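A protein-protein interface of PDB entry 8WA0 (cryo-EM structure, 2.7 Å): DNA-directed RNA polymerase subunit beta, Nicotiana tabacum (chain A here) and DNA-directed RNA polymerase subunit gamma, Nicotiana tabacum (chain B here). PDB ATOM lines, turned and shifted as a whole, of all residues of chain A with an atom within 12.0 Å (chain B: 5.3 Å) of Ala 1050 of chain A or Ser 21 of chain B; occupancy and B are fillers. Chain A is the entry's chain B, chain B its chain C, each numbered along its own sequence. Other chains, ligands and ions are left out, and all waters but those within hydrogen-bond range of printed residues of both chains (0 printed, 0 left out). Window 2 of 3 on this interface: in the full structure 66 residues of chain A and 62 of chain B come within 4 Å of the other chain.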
ATOM      1  N   LEU A1041     -30.704   2.770 -12.647  1.00  0.00           N
ATOM      2  CA  LEU A1041     -29.327   3.115 -12.358  1.00  0.00           C
ATOM      3  C   LEU A1041     -28.983   2.887 -10.914  1.00  0.00           C
ATOM      4  O   LEU A1041     -27.897   2.432 -10.604  1.00  0.00           O
ATOM      5  CB  LEU A1041     -29.052   4.565 -12.699  1.00  0.00           C
ATOM      6  CG  LEU A1041     -28.242   4.855 -13.956  1.00  0.00           C
ATOM      7  CD1 LEU A1041     -28.825   4.143 -15.164  1.00  0.00           C
ATOM      8  CD2 LEU A1041     -28.191   6.355 -14.183  1.00  0.00           C
ATOM      9  N   LEU A1042     -29.891   3.213 -10.014  1.00  0.00           N
ATOM     10  CA  LEU A1042     -29.596   3.075  -8.607  1.00  0.00           C
ATOM     11  C   LEU A1042     -29.347   1.625  -8.297  1.00  0.00           C
ATOM     12  O   LEU A1042     -28.434   1.295  -7.566  1.00  0.00           O
ATOM     13  CB  LEU A1042     -30.747   3.586  -7.766  1.00  0.00           C
ATOM     14  CG  LEU A1042     -30.582   3.585  -6.254  1.00  0.00           C
ATOM     15  CD1 LEU A1042     -29.507   4.576  -5.844  1.00  0.00           C
ATOM     16  CD2 LEU A1042     -31.910   3.934  -5.608  1.00  0.00           C
ATOM     17  N   VAL A1043     -30.146   0.747  -8.872  1.00  0.00           N
ATOM     18  CA  VAL A1043     -29.983  -0.647  -8.587  1.00  0.00           C
ATOM     19  C   VAL A1043     -28.619  -1.089  -9.052  1.00  0.00           C
ATOM     20  O   VAL A1043     -27.912  -1.769  -8.332  1.00  0.00           O
ATOM     21  CB  VAL A1043     -31.048  -1.470  -9.306  1.00  0.00           C
ATOM     22  CG1 VAL A1043     -30.832  -2.953  -9.076  1.00  0.00           C
ATOM     23  CG2 VAL A1043     -32.429  -1.057  -8.838  1.00  0.00           C
ATOM     24  N   ARG A1044     -28.222  -0.670 -10.241  1.00  0.00           N
ATOM     25  CA  ARG A1044     -26.948  -1.091 -10.778  1.00  0.00           C
ATOM     26  C   ARG A1044     -25.803  -0.576  -9.947  1.00  0.00           C
ATOM     27  O   ARG A1044     -24.830  -1.273  -9.725  1.00  0.00           O
ATOM     28  CB  ARG A1044     -26.782  -0.656 -12.216  1.00  0.00           C
ATOM     29  CG  ARG A1044     -27.803  -1.223 -13.172  1.00  0.00           C
ATOM     30  CD  ARG A1044     -27.799  -2.736 -13.142  1.00  0.00           C
ATOM     31  NE  ARG A1044     -28.659  -3.279 -14.183  1.00  0.00           N
ATOM     32  CZ  ARG A1044     -29.963  -3.477 -14.043  1.00  0.00           C
ATOM     33  NH1 ARG A1044     -30.562  -3.178 -12.900  1.00  0.00           N
ATOM     34  NH2 ARG A1044     -30.670  -3.973 -15.045  1.00  0.00           N
ATOM     35  N   GLU A1045     -25.898   0.656  -9.493  1.00  0.00           N
ATOM     36  CA  GLU A1045     -24.856   1.197  -8.653  1.00  0.00           C
ATOM     37  C   GLU A1045     -24.746   0.468  -7.339  1.00  0.00           C
ATOM     38  O   GLU A1045     -23.656   0.208  -6.860  1.00  0.00           O
ATOM     39  CB  GLU A1045     -25.094   2.667  -8.392  1.00  0.00           C
ATOM     40  CG  GLU A1045     -23.831   3.455  -8.084  1.00  0.00           C
ATOM     41  CD  GLU A1045     -23.646   3.726  -6.604  1.00  0.00           C
ATOM     42  OE1 GLU A1045     -24.522   3.324  -5.813  1.00  0.00           O
ATOM     43  OE2 GLU A1045     -22.625   4.342  -6.234  1.00  0.00           O
ATOM     44  N   LEU A1046     -25.870   0.151  -6.733  1.00  0.00           N
ATOM     45  CA  LEU A1046     -25.836  -0.595  -5.500  1.00  0.00           C
ATOM     46  C   LEU A1046     -25.280  -1.985  -5.708  1.00  0.00           C
ATOM     47  O   LEU A1046     -24.534  -2.484  -4.883  1.00  0.00           O
ATOM     48  CB  LEU A1046     -27.209  -0.639  -4.859  1.00  0.00           C
ATOM     49  CG  LEU A1046     -27.705   0.704  -4.336  1.00  0.00           C
ATOM     50  CD1 LEU A1046     -29.056   0.536  -3.667  1.00  0.00           C
ATOM     51  CD2 LEU A1046     -26.696   1.292  -3.366  1.00  0.00           C
ATOM     52  N   ARG A1047     -25.655  -2.618  -6.807  1.00  0.00           N
ATOM     53  CA  ARG A1047     -25.176  -3.956  -7.054  1.00  0.00           C
ATOM     54  C   ARG A1047     -23.697  -3.894  -7.268  1.00  0.00           C
ATOM     55  O   ARG A1047     -23.030  -4.913  -7.219  1.00  0.00           O
ATOM     56  CB  ARG A1047     -25.947  -4.700  -8.141  1.00  0.00           C
ATOM     57  CG  ARG A1047     -25.736  -4.289  -9.569  1.00  0.00           C
ATOM     58  CD  ARG A1047     -26.533  -5.220 -10.460  1.00  0.00           C
ATOM     59  NE  ARG A1047     -27.828  -5.547  -9.880  1.00  0.00           N
ATOM     60  CZ  ARG A1047     -28.721  -6.340 -10.460  1.00  0.00           C
ATOM     61  NH1 ARG A1047     -29.877  -6.588  -9.865  1.00  0.00           N
ATOM     62  NH2 ARG A1047     -28.457  -6.882 -11.637  1.00  0.00           N
ATOM     63  N   SER A1048     -23.164  -2.700  -7.490  1.00  0.00           N
ATOM     64  CA  SER A1048     -21.706  -2.572  -7.549  1.00  0.00           C
ATOM     65  C   SER A1048     -21.011  -2.538  -6.190  1.00  0.00           C
ATOM     66  O   SER A1048     -19.815  -2.742  -6.105  1.00  0.00           O
ATOM     67  CB  SER A1048     -21.313  -1.349  -8.349  1.00  0.00           C
ATOM     68  OG  SER A1048     -19.917  -1.202  -8.433  1.00  0.00           O
ATOM     69  N   LEU A1049     -21.732  -2.217  -5.136  1.00  0.00           N
ATOM     70  CA  LEU A1049     -21.162  -2.166  -3.807  1.00  0.00           C
ATOM     71  C   LEU A1049     -21.595  -3.412  -3.108  1.00  0.00           C
ATOM     72  O   LEU A1049     -21.595  -3.451  -1.893  1.00  0.00           O
ATOM     73  CB  LEU A1049     -21.646  -0.965  -3.027  1.00  0.00           C
ATOM     74  CG  LEU A1049     -21.327   0.426  -3.528  1.00  0.00           C
ATOM     75  CD1 LEU A1049     -22.419   1.365  -3.056  1.00  0.00           C
ATOM     76  CD2 LEU A1049     -19.980   0.850  -2.982  1.00  0.00           C
ATOM     77  N   ALA A1050     -22.024  -4.405  -3.878  1.00  0.00           N
ATOM     78  CA  ALA A1050     -22.464  -5.688  -3.328  1.00  0.00           C
ATOM     79  C   ALA A1050     -23.735  -5.698  -2.494  1.00  0.00           C
ATOM     80  O   ALA A1050     -23.794  -6.396  -1.488  1.00  0.00           O
ATOM     81  CB  ALA A1050     -21.341  -6.365  -2.579  1.00  0.00           C
ATOM     82  N   LEU A1051     -24.759  -4.956  -2.901  1.00  0.00           N
ATOM     83  CA  LEU A1051     -26.031  -4.973  -2.199  1.00  0.00           C
ATOM     84  C   LEU A1051     -27.106  -5.170  -3.242  1.00  0.00           C
ATOM     85  O   LEU A1051     -26.933  -4.753  -4.370  1.00  0.00           O
ATOM     86  CB  LEU A1051     -26.259  -3.659  -1.487  1.00  0.00           C
ATOM     87  CG  LEU A1051     -25.149  -3.029  -0.655  1.00  0.00           C
ATOM     88  CD1 LEU A1051     -25.559  -1.623  -0.256  1.00  0.00           C
ATOM     89  CD2 LEU A1051     -24.851  -3.872   0.570  1.00  0.00           C
ATOM     90  N   GLU A1052     -28.214  -5.799  -2.892  1.00  0.00           N
ATOM     91  CA  GLU A1052     -29.251  -6.081  -3.866  1.00  0.00           C
ATOM     92  C   GLU A1052     -30.576  -5.451  -3.508  1.00  0.00           C
ATOM     93  O   GLU A1052     -31.029  -5.596  -2.386  1.00  0.00           O
ATOM     94  CB  GLU A1052     -29.451  -7.577  -3.935  1.00  0.00           C
ATOM     95  CG  GLU A1052     -30.415  -8.045  -5.002  1.00  0.00           C
ATOM     96  CD  GLU A1052     -30.761  -9.507  -4.837  1.00  0.00           C
ATOM     97  OE1 GLU A1052     -30.522 -10.049  -3.738  1.00  0.00           O
ATOM     98  OE2 GLU A1052     -31.280 -10.111  -5.799  1.00  0.00           O
ATOM     99  N   LEU A1053     -31.211  -4.759  -4.445  1.00  0.00           N
ATOM    100  CA  LEU A1053     -32.527  -4.190  -4.205  1.00  0.00           C
ATOM    101  C   LEU A1053     -33.510  -4.787  -5.180  1.00  0.00           C
ATOM    102  O   LEU A1053     -33.263  -4.785  -6.374  1.00  0.00           O
ATOM    103  CB  LEU A1053     -32.501  -2.690  -4.419  1.00  0.00           C
ATOM    104  CG  LEU A1053     -32.749  -1.766  -3.234  1.00  0.00           C
ATOM    105  CD1 LEU A1053     -32.928  -0.352  -3.754  1.00  0.00           C
ATOM    106  CD2 LEU A1053     -33.984  -2.202  -2.470  1.00  0.00           C
ATOM    107  N   ASN A1054     -34.636  -5.280  -4.689  1.00  0.00           N
ATOM    108  CA  ASN A1054     -35.631  -5.898  -5.551  1.00  0.00           C
ATOM    109  C   ASN A1054     -37.002  -5.330  -5.280  1.00  0.00           C
ATOM    110  O   ASN A1054     -37.287  -4.930  -4.167  1.00  0.00           O
ATOM    111  CB  ASN A1054     -35.681  -7.390  -5.301  1.00  0.00           C
ATOM    112  CG  ASN A1054     -34.436  -8.109  -5.755  1.00  0.00           C
ATOM    113  OD1 ASN A1054     -33.889  -7.826  -6.818  1.00  0.00           O
ATOM    114  ND2 ASN A1054     -33.995  -9.070  -4.958  1.00  0.00           N
ATOM    115  N   PHE A1056     -41.032  -6.205  -5.480  1.00  0.00           N
ATOM    116  CA  PHE A1056     -41.966  -7.284  -5.668  1.00  0.00           C
ATOM    117  C   PHE A1056     -43.369  -6.777  -5.489  1.00  0.00           C
ATOM    118  O   PHE A1056     -43.588  -5.862  -4.711  1.00  0.00           O
ATOM    119  CB  PHE A1056     -41.768  -8.355  -4.614  1.00  0.00           C
ATOM    120  CG  PHE A1056     -40.403  -8.954  -4.575  1.00  0.00           C
ATOM    121  CD1 PHE A1056     -40.056  -9.965  -5.441  1.00  0.00           C
ATOM    122  CD2 PHE A1056     -39.489  -8.550  -3.623  1.00  0.00           C
ATOM    123  CE1 PHE A1056     -38.805 -10.539  -5.389  1.00  0.00           C
ATOM    124  CE2 PHE A1056     -38.237  -9.117  -3.563  1.00  0.00           C
ATOM    125  CZ  PHE A1056     -37.893 -10.114  -4.450  1.00  0.00           C
ATOM    126  N   ARG A1067     -41.793 -10.656  -9.249  1.00  0.00           N
ATOM    127  CA  ARG A1067     -40.670  -9.747  -9.177  1.00  0.00           C
ATOM    128  C   ARG A1067     -40.593  -8.897 -10.403  1.00  0.00           C
ATOM    129  O   ARG A1067     -40.350  -9.403 -11.488  1.00  0.00           O
ATOM    130  CB  ARG A1067     -39.371 -10.527  -9.075  1.00  0.00           C
ATOM    131  CG  ARG A1067     -38.138  -9.640  -9.060  1.00  0.00           C
ATOM    132  CD  ARG A1067     -36.859 -10.450  -9.136  1.00  0.00           C
ATOM    133  NE  ARG A1067     -36.751 -11.383  -8.024  1.00  0.00           N
ATOM    134  CZ  ARG A1067     -35.677 -12.123  -7.776  1.00  0.00           C
ATOM    135  NH1 ARG A1067     -34.615 -12.030  -8.562  1.00  0.00           N
ATOM    136  NH2 ARG A1067     -35.662 -12.950  -6.740  1.00  0.00           N
ATOM    137  N   ILE B  19     -33.857  -5.075   0.585  1.00  0.00           N
ATOM    138  CA  ILE B  19     -32.433  -4.840   0.408  1.00  0.00           C
ATOM    139  C   ILE B  19     -31.643  -5.899   1.149  1.00  0.00           C
ATOM    140  O   ILE B  19     -31.994  -6.274   2.257  1.00  0.00           O
ATOM    141  CB  ILE B  19     -32.024  -3.437   0.881  1.00  0.00           C
ATOM    142  CG1 ILE B  19     -30.552  -3.162   0.580  1.00  0.00           C
ATOM    143  CG2 ILE B  19     -32.337  -3.229   2.353  1.00  0.00           C
ATOM    144  CD1 ILE B  19     -30.102  -1.782   1.000  1.00  0.00           C
ATOM    145  N   GLY B  20     -30.608  -6.434   0.523  1.00  0.00           N
ATOM    146  CA  GLY B  20     -29.834  -7.478   1.158  1.00  0.00           C
ATOM    147  C   GLY B  20     -28.450  -7.648   0.599  1.00  0.00           C
ATOM    148  O   GLY B  20     -28.221  -7.334  -0.555  1.00  0.00           O
ATOM    149  N   SER B  21     -27.521  -8.142   1.402  1.00  0.00           N
ATOM    150  CA  SER B  21     -26.168  -8.375   0.953  1.00  0.00           C
ATOM    151  C   SER B  21     -26.170  -9.612   0.124  1.00  0.00           C
ATOM    152  O   SER B  21     -27.011 -10.468   0.335  1.00  0.00           O
ATOM    153  CB  SER B  21     -25.208  -8.481   2.127  1.00  0.00           C
ATOM    154  OG  SER B  21     -23.859  -8.495   1.707  1.00  0.00           O
ATOM    155  N   VAL B  22     -25.249  -9.747  -0.817  1.00  0.00           N
ATOM    156  CA  VAL B  22     -25.309 -10.872  -1.725  1.00  0.00           C
ATOM    157  C   VAL B  22     -24.183 -11.853  -1.691  1.00  0.00           C
ATOM    158  O   VAL B  22     -23.042 -11.486  -1.467  1.00  0.00           O
ATOM    159  CB  VAL B  22     -25.480 -10.429  -3.170  1.00  0.00           C
ATOM    160  CG1 VAL B  22     -26.936 -10.202  -3.497  1.00  0.00           C
ATOM    161  CG2 VAL B  22     -24.636  -9.203  -3.454  1.00  0.00           C
ATOM    162  N   SER B  23     -24.501 -13.115  -1.923  1.00  0.00           N
ATOM    163  CA  SER B  23     -23.517 -14.182  -1.918  1.00  0.00           C
ATOM    164  C   SER B  23     -22.634 -14.203  -3.131  1.00  0.00           C
ATOM    165  O   SER B  23     -22.992 -13.682  -4.170  1.00  0.00           O
ATOM    166  CB  SER B  23     -24.269 -15.494  -1.896  1.00  0.00           C
ATOM    167  OG  SER B  23     -24.975 -15.675  -3.107  1.00  0.00           O
ATOM    168  N   HIS B 122     -15.014  -5.771   3.243  1.00  0.00           N
ATOM    169  CA  HIS B 122     -15.759  -4.538   2.979  1.00  0.00           C
ATOM    170  C   HIS B 122     -15.459  -3.539   4.039  1.00  0.00           C
ATOM    171  O   HIS B 122     -15.465  -3.875   5.209  1.00  0.00           O
ATOM    172  CB  HIS B 122     -17.249  -4.842   3.075  1.00  0.00           C
ATOM    173  CG  HIS B 122     -18.125  -3.981   2.211  1.00  0.00           C
ATOM    174  ND1 HIS B 122     -18.033  -2.608   2.177  1.00  0.00           N
ATOM    175  CD2 HIS B 122     -19.137  -4.307   1.371  1.00  0.00           C
ATOM    176  CE1 HIS B 122     -18.932  -2.128   1.338  1.00  0.00           C
ATOM    177  NE2 HIS B 122     -19.614  -3.139   0.834  1.00  0.00           N
ATOM    178  N   TYR B 125     -18.642  -2.420   7.337  1.00  0.00           N
ATOM    179  CA  TYR B 125     -18.831  -3.204   8.539  1.00  0.00           C
ATOM    180  C   TYR B 125     -17.690  -2.926   9.503  1.00  0.00           C
ATOM    181  O   TYR B 125     -17.926  -2.714  10.686  1.00  0.00           O
ATOM    182  CB  TYR B 125     -18.917  -4.689   8.190  1.00  0.00           C
ATOM    183  CG  TYR B 125     -19.982  -4.999   7.162  1.00  0.00           C
ATOM    184  CD1 TYR B 125     -21.299  -5.217   7.542  1.00  0.00           C
ATOM    185  CD2 TYR B 125     -19.674  -5.066   5.810  1.00  0.00           C
ATOM    186  CE1 TYR B 125     -22.276  -5.496   6.607  1.00  0.00           C
ATOM    187  CE2 TYR B 125     -20.645  -5.343   4.867  1.00  0.00           C
ATOM    188  CZ  TYR B 125     -21.944  -5.559   5.271  1.00  0.00           C
ATOM    189  OH  TYR B 125     -22.915  -5.837   4.336  1.00  0.00           O
ATOM    190  N   ILE B 266     -29.532 -14.175   5.472  1.00  0.00           N
ATOM    191  CA  ILE B 266     -28.307 -13.555   4.989  1.00  0.00           C
ATOM    192  C   ILE B 266     -27.166 -14.242   5.714  1.00  0.00           C
ATOM    193  O   ILE B 266     -27.202 -14.355   6.931  1.00  0.00           O
ATOM    194  CB  ILE B 266     -28.279 -12.056   5.321  1.00  0.00           C
ATOM    195  CG1 ILE B 266     -29.438 -11.332   4.643  1.00  0.00           C
ATOM    196  CG2 ILE B 266     -26.962 -11.428   4.899  1.00  0.00           C
ATOM    197  CD1 ILE B 266     -29.338 -11.321   3.136  1.00  0.00           C
ATOM    198  N   TRP B 270     -20.581 -13.517   4.050  1.00  0.00           N
ATOM    199  CA  TRP B 270     -20.613 -12.755   2.839  1.00  0.00           C
ATOM    200  C   TRP B 270     -19.954 -11.388   2.990  1.00  0.00           C
ATOM    201  O   TRP B 270     -19.680 -10.729   1.996  1.00  0.00           O
ATOM    202  CB  TRP B 270     -22.029 -12.627   2.352  1.00  0.00           C
ATOM    203  CG  TRP B 270     -22.708 -13.898   2.025  1.00  0.00           C
ATOM    204  CD1 TRP B 270     -22.133 -15.106   1.800  1.00  0.00           C
ATOM    205  CD2 TRP B 270     -24.113 -14.085   1.862  1.00  0.00           C
ATOM    206  NE1 TRP B 270     -23.094 -16.041   1.517  1.00  0.00           N
ATOM    207  CE2 TRP B 270     -24.320 -15.435   1.550  1.00  0.00           C
ATOM    208  CE3 TRP B 270     -25.216 -13.240   1.955  1.00  0.00           C
ATOM    209  CZ2 TRP B 270     -25.584 -15.958   1.328  1.00  0.00           C
ATOM    210  CZ3 TRP B 270     -26.462 -13.759   1.735  1.00  0.00           C
ATOM    211  CH2 TRP B 270     -26.640 -15.103   1.428  1.00  0.00           C
ATOM    212  N   LEU B 273     -15.291 -10.573   0.867  1.00  0.00           N
ATOM    213  CA  LEU B 273     -15.704 -10.837  -0.493  1.00  0.00           C
ATOM    214  C   LEU B 273     -14.860 -11.638  -1.409  1.00  0.00           C
ATOM    215  O   LEU B 273     -13.732 -11.269  -1.698  1.00  0.00           O
ATOM    216  CB  LEU B 273     -15.833  -9.474  -1.190  1.00  0.00           C
ATOM    217  CG  LEU B 273     -16.749  -8.359  -0.680  1.00  0.00           C
ATOM    218  CD1 LEU B 273     -16.003  -7.406   0.235  1.00  0.00           C
ATOM    219  CD2 LEU B 273     -17.279  -7.584  -1.869  1.00  0.00           C
ATOM    220  N   PRO B 277     -17.960  -7.260  -8.089  1.00  0.00           N
ATOM    221  CA  PRO B 277     -18.827  -6.761  -9.167  1.00  0.00           C
ATOM    222  C   PRO B 277     -18.301  -5.614 -10.033  1.00  0.00           C
ATOM    223  O   PRO B 277     -17.529  -4.819  -9.533  1.00  0.00           O
ATOM    224  CB  PRO B 277     -20.035  -6.254  -8.407  1.00  0.00           C
ATOM    225  CG  PRO B 277     -19.915  -6.729  -7.006  1.00  0.00           C
ATOM    226  CD  PRO B 277     -18.470  -6.904  -6.759  1.00  0.00           C
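The backbone NH (N) of Leu 1051 of chain A lies within hydrogen-bond range of the backbone carbonyl oxygen (O) of Leu 1046 of chain A.
The side-chain carboxylate (OE2) of Glu 1052 of chain A sits at hydrogen-bond distance from the side-chain amide nitrogen (ND2) of Asn 1054 of chain A, 3.0 Å away.
Among the printed residues, 8 pairs touch across the chains.
Among the printed residues, no Asp or Glu carboxylate lies within 4 Å of a Lys or Arg side-chain nitrogen of the other chain.
The backbone carbonyl oxygen (O) of Leu 1049 of chain A is in hydrogen-bond range of a ring nitrogen (NE2) of His 122 of chain B, at 3.4 Å.
The backbone NH (N) of Glu 1052 of chain A sits at hydrogen-bond distance from the backbone carbonyl oxygen (O) of Gly 20 of chain B (2.8 Å).
Of the printed residues of chain B, Arg 1047 of chain A touches Pro 277.
Of the printed residues of chain B, Leu 1049 of chain A touches His 122.
Ala 1050 of chain A touches just these residues of chain B: Ser 21 and Val 22.
Of the printed residues of chain B, Leu 1051 of chain A touches Gly 20.
Of the printed residues of chain B, Glu 1052 of chain A touches Ile 19 (3.2 Å), Gly 20 (2.8 Å) and Val 22 (3.6 Å).
Ile 19 of chain B touches one residue of chain A.
Ser 21 of chain B touches just one residue of chain A: Ala 1050 (3.8 Å).
Of chain A, only Ala 1050 (3.5 Å) and Glu 1052 (3.6 Å) come within 4 Å of Val 22 of chain B.
No residue of chain A comes within 4 Å of Ser 23 of chain B.
Of the printed residues of chain A, His 122 of chain B touches Leu 1049 (3.4 Å).
No residue of chain A comes within 4 Å of Ile 266 of chain B.
No residue of chain A comes within 4 Å of Trp 270 of chain B.
The nearest residue of chain A that does not touch Ser 21 of chain B is Leu 1051 of chain A (4.6 Å).
The nearest printed residue of chain B that does not touch Leu 1051 of chain A is Val 22 of chain B (4.3 Å).
Among the printed residues, pairs that only touch across the chains: Arg 1047 of chain A with Pro 277 of chain B, Ala 1050 of chain A with Ser 21 of chain B, Ala 1050 of chain A with Val 22 of chain B, Leu 1051 of chain A with Gly 20 of chain B, Glu 1052 of chain A with Ile 19 of chain B and Glu 1052 of chain A with Val 22 of chain B.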
